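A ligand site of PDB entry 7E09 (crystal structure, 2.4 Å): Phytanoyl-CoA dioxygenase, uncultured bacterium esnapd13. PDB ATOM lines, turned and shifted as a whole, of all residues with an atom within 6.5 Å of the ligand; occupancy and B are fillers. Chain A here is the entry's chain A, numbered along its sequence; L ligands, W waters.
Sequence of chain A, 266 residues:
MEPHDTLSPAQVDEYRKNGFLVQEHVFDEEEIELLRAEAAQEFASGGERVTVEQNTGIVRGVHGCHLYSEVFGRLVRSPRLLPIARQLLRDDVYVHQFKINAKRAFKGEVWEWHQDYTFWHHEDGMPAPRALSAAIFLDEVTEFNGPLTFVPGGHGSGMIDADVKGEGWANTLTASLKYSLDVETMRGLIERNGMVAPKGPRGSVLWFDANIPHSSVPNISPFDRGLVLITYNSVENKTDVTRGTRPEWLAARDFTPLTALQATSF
NH1 of Arg 246 lies within hydrogen-bond range of OG1 of Thr 172 (3.4 Å). NH2 of Arg 246 sits close to NE2 of Gln 97 (3.5 Å). OD1 of Asp 124 lies within salt-bridge range of NE of Arg 246 (2.8 Å). The side-chain amide oxygen of Gln 97 lies within hydrogen-bond range of the side-chain amino group of Lys 99 (2.7 Å). NE2 of Gln 97 sits at hydrogen-bond distance from O of Leu 250, at 2.9 Å. The backbone carbonyl oxygen (O) of Gln 97 is in hydrogen-bond range of the backbone NH (N) of Thr 231, at 2.8 Å. O of His 114 sits at hydrogen-bond distance from N of His 214, at 2.9 Å.
Residues that only touch the ligand: His 114 (3.9 Å) and Phe 119 (3.2 Å). Hydrophobic or aromatic side chains that line the ligand: His 114, Phe 119 and Trp 120. Along chain A the residues within 4 Å of the ligand span positions 97 to 246.
Water W1 lies within hydrogen-bond range of NZ of Lys 99, OD2 of Asp 116, OG of Ser 133 and O2 of the ligand.
An oxygen (O2) of the ligand lies within hydrogen-bond range of the side-chain carboxylate (OD1) of Asp 116, at 2.7 Å. An oxygen (O1) of the ligand lies within salt-bridge range of the guanidinium group (NH2) of Arg 246 (3.0 Å). O of Thr 172 lies within hydrogen-bond range of N1 of the ligand (3.1 Å). NE2 of Gln 97 is in hydrogen-bond range of O1 of the ligand (3.1 Å). NE1 of Trp 120 is in hydrogen-bond range of O1 of the ligand. The side-chain amino group of Lys 99 lies within hydrogen-bond range of an oxygen (O2) of the ligand (3.2 Å).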
ATOM      1  N   HIS A  63      24.835  -7.784   3.810  1.00  0.00           N
ATOM      2  CA  HIS A  63      23.763  -6.866   3.484  1.00  0.00           C
ATOM      3  C   HIS A  63      22.540  -7.541   2.790  1.00  0.00           C
ATOM      4  O   HIS A  63      22.712  -8.444   1.959  1.00  0.00           O
ATOM      5  CB  HIS A  63      24.333  -5.735   2.632  1.00  0.00           C
ATOM      6  CG  HIS A  63      25.119  -4.746   3.425  1.00  0.00           C
ATOM      7  ND1 HIS A  63      26.384  -5.016   3.909  1.00  0.00           N
ATOM      8  CD2 HIS A  63      24.805  -3.505   3.868  1.00  0.00           C
ATOM      9  CE1 HIS A  63      26.812  -3.978   4.604  1.00  0.00           C
ATOM     10  NE2 HIS A  63      25.881  -3.044   4.585  1.00  0.00           N
ATOM     11  N   HIS A  96      14.324  -0.446   4.801  1.00  0.00           N
ATOM     12  CA  HIS A  96      15.249   0.135   3.809  1.00  0.00           C
ATOM     13  C   HIS A  96      16.545  -0.673   3.602  1.00  0.00           C
ATOM     14  O   HIS A  96      17.018  -0.871   2.460  1.00  0.00           O
ATOM     15  CB  HIS A  96      15.553   1.523   4.297  1.00  0.00           C
ATOM     16  CG  HIS A  96      16.604   2.223   3.513  1.00  0.00           C
ATOM     17  ND1 HIS A  96      16.483   2.464   2.167  1.00  0.00           N
ATOM     18  CD2 HIS A  96      17.786   2.773   3.899  1.00  0.00           C
ATOM     19  CE1 HIS A  96      17.558   3.099   1.746  1.00  0.00           C
ATOM     20  NE2 HIS A  96      18.361   3.306   2.782  1.00  0.00           N
ATOM     21  N   GLN A  97      17.083  -1.196   4.687  1.00  0.00           N
ATOM     22  CA  GLN A  97      18.380  -1.857   4.675  1.00  0.00           C
ATOM     23  C   GLN A  97      18.444  -2.826   5.808  1.00  0.00           C
ATOM     24  O   GLN A  97      18.018  -2.544   6.919  1.00  0.00           O
ATOM     25  CB  GLN A  97      19.489  -0.786   4.871  1.00  0.00           C
ATOM     26  CG  GLN A  97      20.939  -1.292   4.862  1.00  0.00           C
ATOM     27  CD  GLN A  97      21.976  -0.144   4.818  1.00  0.00           C
ATOM     28  OE1 GLN A  97      22.471   0.275   5.860  1.00  0.00           O
ATOM     29  NE2 GLN A  97      22.302   0.347   3.605  1.00  0.00           N
ATOM     30  N   LYS A  99      21.456  -5.393   7.698  1.00  0.00           N
ATOM     31  CA  LYS A  99      22.844  -5.885   7.682  1.00  0.00           C
ATOM     32  C   LYS A  99      23.261  -6.495   8.967  1.00  0.00           C
ATOM     33  O   LYS A  99      22.784  -6.094  10.074  1.00  0.00           O
ATOM     34  CB  LYS A  99      23.808  -4.711   7.346  1.00  0.00           C
ATOM     35  CG  LYS A  99      23.873  -3.582   8.357  1.00  0.00           C
ATOM     36  CD  LYS A  99      24.555  -2.349   7.766  1.00  0.00           C
ATOM     37  CE  LYS A  99      24.405  -1.075   8.602  1.00  0.00           C
ATOM     38  NZ  LYS A  99      23.093  -0.355   8.450  1.00  0.00           N
ATOM     39  N   TRP A 111      35.674   2.750  13.073  1.00  0.00           N
ATOM     40  CA  TRP A 111      34.667   3.248  12.155  1.00  0.00           C
ATOM     41  C   TRP A 111      34.556   4.731  12.429  1.00  0.00           C
ATOM     42  O   TRP A 111      34.027   5.114  13.481  1.00  0.00           O
ATOM     43  CB  TRP A 111      33.307   2.594  12.416  1.00  0.00           C
ATOM     44  CG  TRP A 111      33.177   1.289  11.813  1.00  0.00           C
ATOM     45  CD1 TRP A 111      33.852   0.147  12.155  1.00  0.00           C
ATOM     46  CD2 TRP A 111      32.313   0.943  10.735  1.00  0.00           C
ATOM     47  NE1 TRP A 111      33.449  -0.897  11.344  1.00  0.00           N
ATOM     48  CE2 TRP A 111      32.506  -0.442  10.475  1.00  0.00           C
ATOM     49  CE3 TRP A 111      31.377   1.666   9.973  1.00  0.00           C
ATOM     50  CZ2 TRP A 111      31.792  -1.131   9.465  1.00  0.00           C
ATOM     51  CZ3 TRP A 111      30.659   0.985   8.960  1.00  0.00           C
ATOM     52  CH2 TRP A 111      30.882  -0.399   8.720  1.00  0.00           C
ATOM     53  N   HIS A 114      30.114   9.204  11.656  1.00  0.00           N
ATOM     54  CA  HIS A 114      29.201   9.374  10.502  1.00  0.00           C
ATOM     55  C   HIS A 114      27.727   9.405  10.870  1.00  0.00           C
ATOM     56  O   HIS A 114      27.318   9.112  12.022  1.00  0.00           O
ATOM     57  CB  HIS A 114      29.405   8.288   9.467  1.00  0.00           C
ATOM     58  CG  HIS A 114      29.102   6.928   9.976  1.00  0.00           C
ATOM     59  ND1 HIS A 114      29.809   6.345  11.011  1.00  0.00           N
ATOM     60  CD2 HIS A 114      28.151   6.031   9.615  1.00  0.00           C
ATOM     61  CE1 HIS A 114      29.319   5.138  11.254  1.00  0.00           C
ATOM     62  NE2 HIS A 114      28.313   4.928  10.424  1.00  0.00           N
ATOM     63  N   GLN A 115      26.948   9.816   9.887  1.00  0.00           N
ATOM     64  CA  GLN A 115      25.478   9.842   9.969  1.00  0.00           C
ATOM     65  C   GLN A 115      24.949   8.981   8.866  1.00  0.00           C
ATOM     66  O   GLN A 115      25.261   9.259   7.737  1.00  0.00           O
ATOM     67  CB  GLN A 115      24.964  11.241   9.776  1.00  0.00           C
ATOM     68  CG  GLN A 115      25.135  12.103  11.006  1.00  0.00           C
ATOM     69  CD  GLN A 115      24.945  13.588  10.698  1.00  0.00           C
ATOM     70  OE1 GLN A 115      25.478  14.081   9.692  1.00  0.00           O
ATOM     71  NE2 GLN A 115      24.205  14.275  11.540  1.00  0.00           N
ATOM     72  N   ASP A 116      24.153   7.957   9.180  1.00  0.00           N
ATOM     73  CA  ASP A 116      23.481   7.107   8.175  1.00  0.00           C
ATOM     74  C   ASP A 116      22.649   7.898   7.194  1.00  0.00           C
ATOM     75  O   ASP A 116      22.712   7.637   6.035  1.00  0.00           O
ATOM     76  CB  ASP A 116      22.530   6.122   8.852  1.00  0.00           C
ATOM     77  CG  ASP A 116      23.260   5.024   9.622  1.00  0.00           C
ATOM     78  OD1 ASP A 116      24.412   4.709   9.243  1.00  0.00           O
ATOM     79  OD2 ASP A 116      22.686   4.533  10.625  1.00  0.00           O
ATOM     80  N   PHE A 119      24.405   9.223   3.978  1.00  0.00           N
ATOM     81  CA  PHE A 119      24.526   8.220   2.924  1.00  0.00           C
ATOM     82  C   PHE A 119      23.175   7.956   2.251  1.00  0.00           C
ATOM     83  O   PHE A 119      23.098   7.762   1.049  1.00  0.00           O
ATOM     84  CB  PHE A 119      24.951   6.860   3.487  1.00  0.00           C
ATOM     85  CG  PHE A 119      26.355   6.791   3.983  1.00  0.00           C
ATOM     86  CD1 PHE A 119      26.712   7.309   5.244  1.00  0.00           C
ATOM     87  CD2 PHE A 119      27.326   6.120   3.252  1.00  0.00           C
ATOM     88  CE1 PHE A 119      28.028   7.215   5.733  1.00  0.00           C
ATOM     89  CE2 PHE A 119      28.640   6.020   3.730  1.00  0.00           C
ATOM     90  CZ  PHE A 119      28.989   6.560   4.970  1.00  0.00           C
ATOM     91  N   TRP A 120      22.100   7.876   3.018  1.00  0.00           N
ATOM     92  CA  TRP A 120      20.800   7.429   2.442  1.00  0.00           C
ATOM     93  C   TRP A 120      20.178   8.539   1.609  1.00  0.00           C
ATOM     94  O   TRP A 120      19.557   8.277   0.569  1.00  0.00           O
ATOM     95  CB  TRP A 120      19.836   6.931   3.541  1.00  0.00           C
ATOM     96  CG  TRP A 120      20.365   5.703   4.284  1.00  0.00           C
ATOM     97  CD1 TRP A 120      21.167   4.724   3.756  1.00  0.00           C
ATOM     98  CD2 TRP A 120      20.092   5.303   5.650  1.00  0.00           C
ATOM     99  NE1 TRP A 120      21.401   3.744   4.714  1.00  0.00           N
ATOM    100  CE2 TRP A 120      20.784   4.091   5.883  1.00  0.00           C
ATOM    101  CE3 TRP A 120      19.359   5.861   6.698  1.00  0.00           C
ATOM    102  CZ2 TRP A 120      20.733   3.401   7.102  1.00  0.00           C
ATOM    103  CZ3 TRP A 120      19.292   5.176   7.942  1.00  0.00           C
ATOM    104  CH2 TRP A 120      19.996   3.974   8.134  1.00  0.00           C
ATOM    105  N   GLU A 123      22.948   8.687  -1.568  1.00  0.00           N
ATOM    106  CA  GLU A 123      23.042   7.476  -2.365  1.00  0.00           C
ATOM    107  C   GLU A 123      21.679   6.950  -2.837  1.00  0.00           C
ATOM    108  O   GLU A 123      21.606   6.386  -3.941  1.00  0.00           O
ATOM    109  CB  GLU A 123      23.766   6.357  -1.608  1.00  0.00           C
ATOM    110  CG  GLU A 123      25.182   6.697  -1.144  1.00  0.00           C
ATOM    111  CD  GLU A 123      26.159   6.939  -2.303  1.00  0.00           C
ATOM    112  OE1 GLU A 123      26.270   6.062  -3.214  1.00  0.00           O
ATOM    113  OE2 GLU A 123      26.802   8.007  -2.291  1.00  0.00           O
ATOM    114  N   ASP A 124      20.640   7.051  -1.990  1.00  0.00           N
ATOM    115  CA  ASP A 124      19.391   6.321  -2.271  1.00  0.00           C
ATOM    116  C   ASP A 124      18.166   7.208  -2.548  1.00  0.00           C
ATOM    117  O   ASP A 124      17.151   6.707  -3.061  1.00  0.00           O
ATOM    118  CB  ASP A 124      19.053   5.383  -1.128  1.00  0.00           C
ATOM    119  CG  ASP A 124      20.190   4.436  -0.778  1.00  0.00           C
ATOM    120  OD1 ASP A 124      20.888   3.939  -1.666  1.00  0.00           O
ATOM    121  OD2 ASP A 124      20.349   4.164   0.417  1.00  0.00           O
ATOM    122  N   SER A 133      17.354   2.656  13.010  1.00  0.00           N
ATOM    123  CA  SER A 133      17.926   1.335  12.953  1.00  0.00           C
ATOM    124  C   SER A 133      17.701   0.649  14.287  1.00  0.00           C
ATOM    125  O   SER A 133      17.624   1.288  15.329  1.00  0.00           O
ATOM    126  CB  SER A 133      19.354   1.394  12.540  1.00  0.00           C
ATOM    127  OG  SER A 133      19.473   1.848  11.149  1.00  0.00           O
ATOM    128  N   ASN A 171      32.918   2.282  -1.130  1.00  0.00           N
ATOM    129  CA  ASN A 171      33.273   2.506   0.309  1.00  0.00           C
ATOM    130  C   ASN A 171      32.148   3.097   1.215  1.00  0.00           C
ATOM    131  O   ASN A 171      32.393   3.838   2.175  1.00  0.00           O
ATOM    132  CB  ASN A 171      34.664   3.224   0.467  1.00  0.00           C
ATOM    133  CG  ASN A 171      34.671   4.701   0.060  1.00  0.00           C
ATOM    134  OD1 ASN A 171      35.271   5.527   0.745  1.00  0.00           O
ATOM    135  ND2 ASN A 171      34.061   5.037  -1.079  1.00  0.00           N
ATOM    136  N   THR A 172      30.910   2.691   0.903  1.00  0.00           N
ATOM    137  CA  THR A 172      29.748   2.820   1.810  1.00  0.00           C
ATOM    138  C   THR A 172      29.752   1.719   2.913  1.00  0.00           C
ATOM    139  O   THR A 172      29.280   1.924   4.042  1.00  0.00           O
ATOM    140  CB  THR A 172      28.389   2.831   1.004  1.00  0.00           C
ATOM    141  OG1 THR A 172      28.180   1.608   0.275  1.00  0.00           O
ATOM    142  CG2 THR A 172      28.333   4.003   0.024  1.00  0.00           C
ATOM    143  N   LEU A 173      30.317   0.555   2.585  1.00  0.00           N
ATOM    144  CA  LEU A 173      30.224  -0.659   3.389  1.00  0.00           C
ATOM    145  C   LEU A 173      31.435  -0.817   4.326  1.00  0.00           C
ATOM    146  O   LEU A 173      31.338  -1.484   5.367  1.00  0.00           O
ATOM    147  CB  LEU A 173      30.123  -1.880   2.453  1.00  0.00           C
ATOM    148  CG  LEU A 173      29.212  -1.747   1.222  1.00  0.00           C
ATOM    149  CD1 LEU A 173      29.233  -3.009   0.349  1.00  0.00           C
ATOM    150  CD2 LEU A 173      27.813  -1.384   1.708  1.00  0.00           C
ATOM    151  N   THR A 174      32.563  -0.193   3.954  1.00  0.00           N
ATOM    152  CA  THR A 174      33.861  -0.382   4.591  1.00  0.00           C
ATOM    153  C   THR A 174      34.145   0.685   5.695  1.00  0.00           C
ATOM    154  O   THR A 174      33.521   1.748   5.687  1.00  0.00           O
ATOM    155  CB  THR A 174      34.954  -0.346   3.493  1.00  0.00           C
ATOM    156  OG1 THR A 174      34.933   0.924   2.847  1.00  0.00           O
ATOM    157  CG2 THR A 174      34.694  -1.440   2.434  1.00  0.00           C
ATOM    158  N   LEU A 177      35.105   5.502   5.376  1.00  0.00           N
ATOM    159  CA  LEU A 177      33.769   5.831   4.836  1.00  0.00           C
ATOM    160  C   LEU A 177      33.739   7.019   3.860  1.00  0.00           C
ATOM    161  O   LEU A 177      34.499   7.991   3.976  1.00  0.00           O
ATOM    162  CB  LEU A 177      32.795   6.088   6.003  1.00  0.00           C
ATOM    163  CG  LEU A 177      32.362   4.884   6.861  1.00  0.00           C
ATOM    164  CD1 LEU A 177      31.689   5.396   8.124  1.00  0.00           C
ATOM    165  CD2 LEU A 177      31.454   3.929   6.091  1.00  0.00           C
ATOM    166  N   HIS A 214      27.602   8.565  14.813  1.00  0.00           N
ATOM    167  CA  HIS A 214      28.083   7.413  15.560  1.00  0.00           C
ATOM    168  C   HIS A 214      29.347   6.847  15.005  1.00  0.00           C
ATOM    169  O   HIS A 214      29.698   7.044  13.794  1.00  0.00           O
ATOM    170  CB  HIS A 214      26.999   6.313  15.674  1.00  0.00           C
ATOM    171  CG  HIS A 214      26.690   5.611  14.389  1.00  0.00           C
ATOM    172  ND1 HIS A 214      25.899   6.154  13.413  1.00  0.00           N
ATOM    173  CD2 HIS A 214      27.038   4.392  13.928  1.00  0.00           C
ATOM    174  CE1 HIS A 214      25.807   5.336  12.384  1.00  0.00           C
ATOM    175  NE2 HIS A 214      26.474   4.245  12.690  1.00  0.00           N
ATOM    176  N   THR A 231      17.181  -1.401   9.374  1.00  0.00           N
ATOM    177  CA  THR A 231      16.848  -0.042   9.209  1.00  0.00           C
ATOM    178  C   THR A 231      15.387   0.061   8.719  1.00  0.00           C
ATOM    179  O   THR A 231      15.066  -0.304   7.579  1.00  0.00           O
ATOM    180  CB  THR A 231      17.827   0.672   8.255  1.00  0.00           C
ATOM    181  OG1 THR A 231      19.141   0.747   8.862  1.00  0.00           O
ATOM    182  CG2 THR A 231      17.378   2.093   8.089  1.00  0.00           C
ATOM    183  N   ARG A 246      22.157   2.498  -5.817  1.00  0.00           N
ATOM    184  CA  ARG A 246      22.581   1.189  -5.250  1.00  0.00           C
ATOM    185  C   ARG A 246      21.570   0.083  -5.497  1.00  0.00           C
ATOM    186  O   ARG A 246      20.497   0.362  -5.941  1.00  0.00           O
ATOM    187  CB  ARG A 246      22.840   1.341  -3.755  1.00  0.00           C
ATOM    188  CG  ARG A 246      23.655   2.571  -3.426  1.00  0.00           C
ATOM    189  CD  ARG A 246      24.278   2.460  -2.073  1.00  0.00           C
ATOM    190  NE  ARG A 246      23.337   2.681  -0.964  1.00  0.00           N
ATOM    191  CZ  ARG A 246      23.676   2.602   0.331  1.00  0.00           C
ATOM    192  NH1 ARG A 246      24.920   2.277   0.701  1.00  0.00           N
ATOM    193  NH2 ARG A 246      22.769   2.842   1.267  1.00  0.00           N
ATOM    194  N   LEU A 250      21.087  -3.273  -0.661  1.00  0.00           N
ATOM    195  CA  LEU A 250      21.540  -2.131   0.168  1.00  0.00           C
ATOM    196  C   LEU A 250      20.445  -1.091   0.458  1.00  0.00           C
ATOM    197  O   LEU A 250      20.468  -0.430   1.514  1.00  0.00           O
ATOM    198  CB  LEU A 250      22.708  -1.396  -0.521  1.00  0.00           C
ATOM    199  CG  LEU A 250      24.045  -2.148  -0.733  1.00  0.00           C
ATOM    200  CD1 LEU A 250      25.067  -1.171  -1.326  1.00  0.00           C
ATOM    201  CD2 LEU A 250      24.573  -2.767   0.565  1.00  0.00           C
HETATM  202  C1  LIG L   1      25.371   2.668   4.334  1.00  0.00           C
HETATM  203  O1  LIG L   1      24.236   2.750   3.831  1.00  0.00           O
HETATM  204  N1  LIG L   1      26.938   1.753   6.032  1.00  0.00           N
HETATM  205  C2  LIG L   1      25.559   2.029   5.677  1.00  0.00           C
HETATM  206  C3  LIG L   1      25.165   3.056   6.717  1.00  0.00           C
HETATM  207  C4  LIG L   1      26.442   3.872   6.894  1.00  0.00           C
HETATM  208  C5  LIG L   1      27.552   2.830   6.759  1.00  0.00           C
HETATM  209  O2  LIG L   1      24.786   2.358   7.916  1.00  0.00           O
HETATM  210  O3  LIG L   1      26.367   3.122   3.757  1.00  0.00           O
HETATM  211  O   HOH W   1      22.525   1.488  10.297  1.00  0.00           O
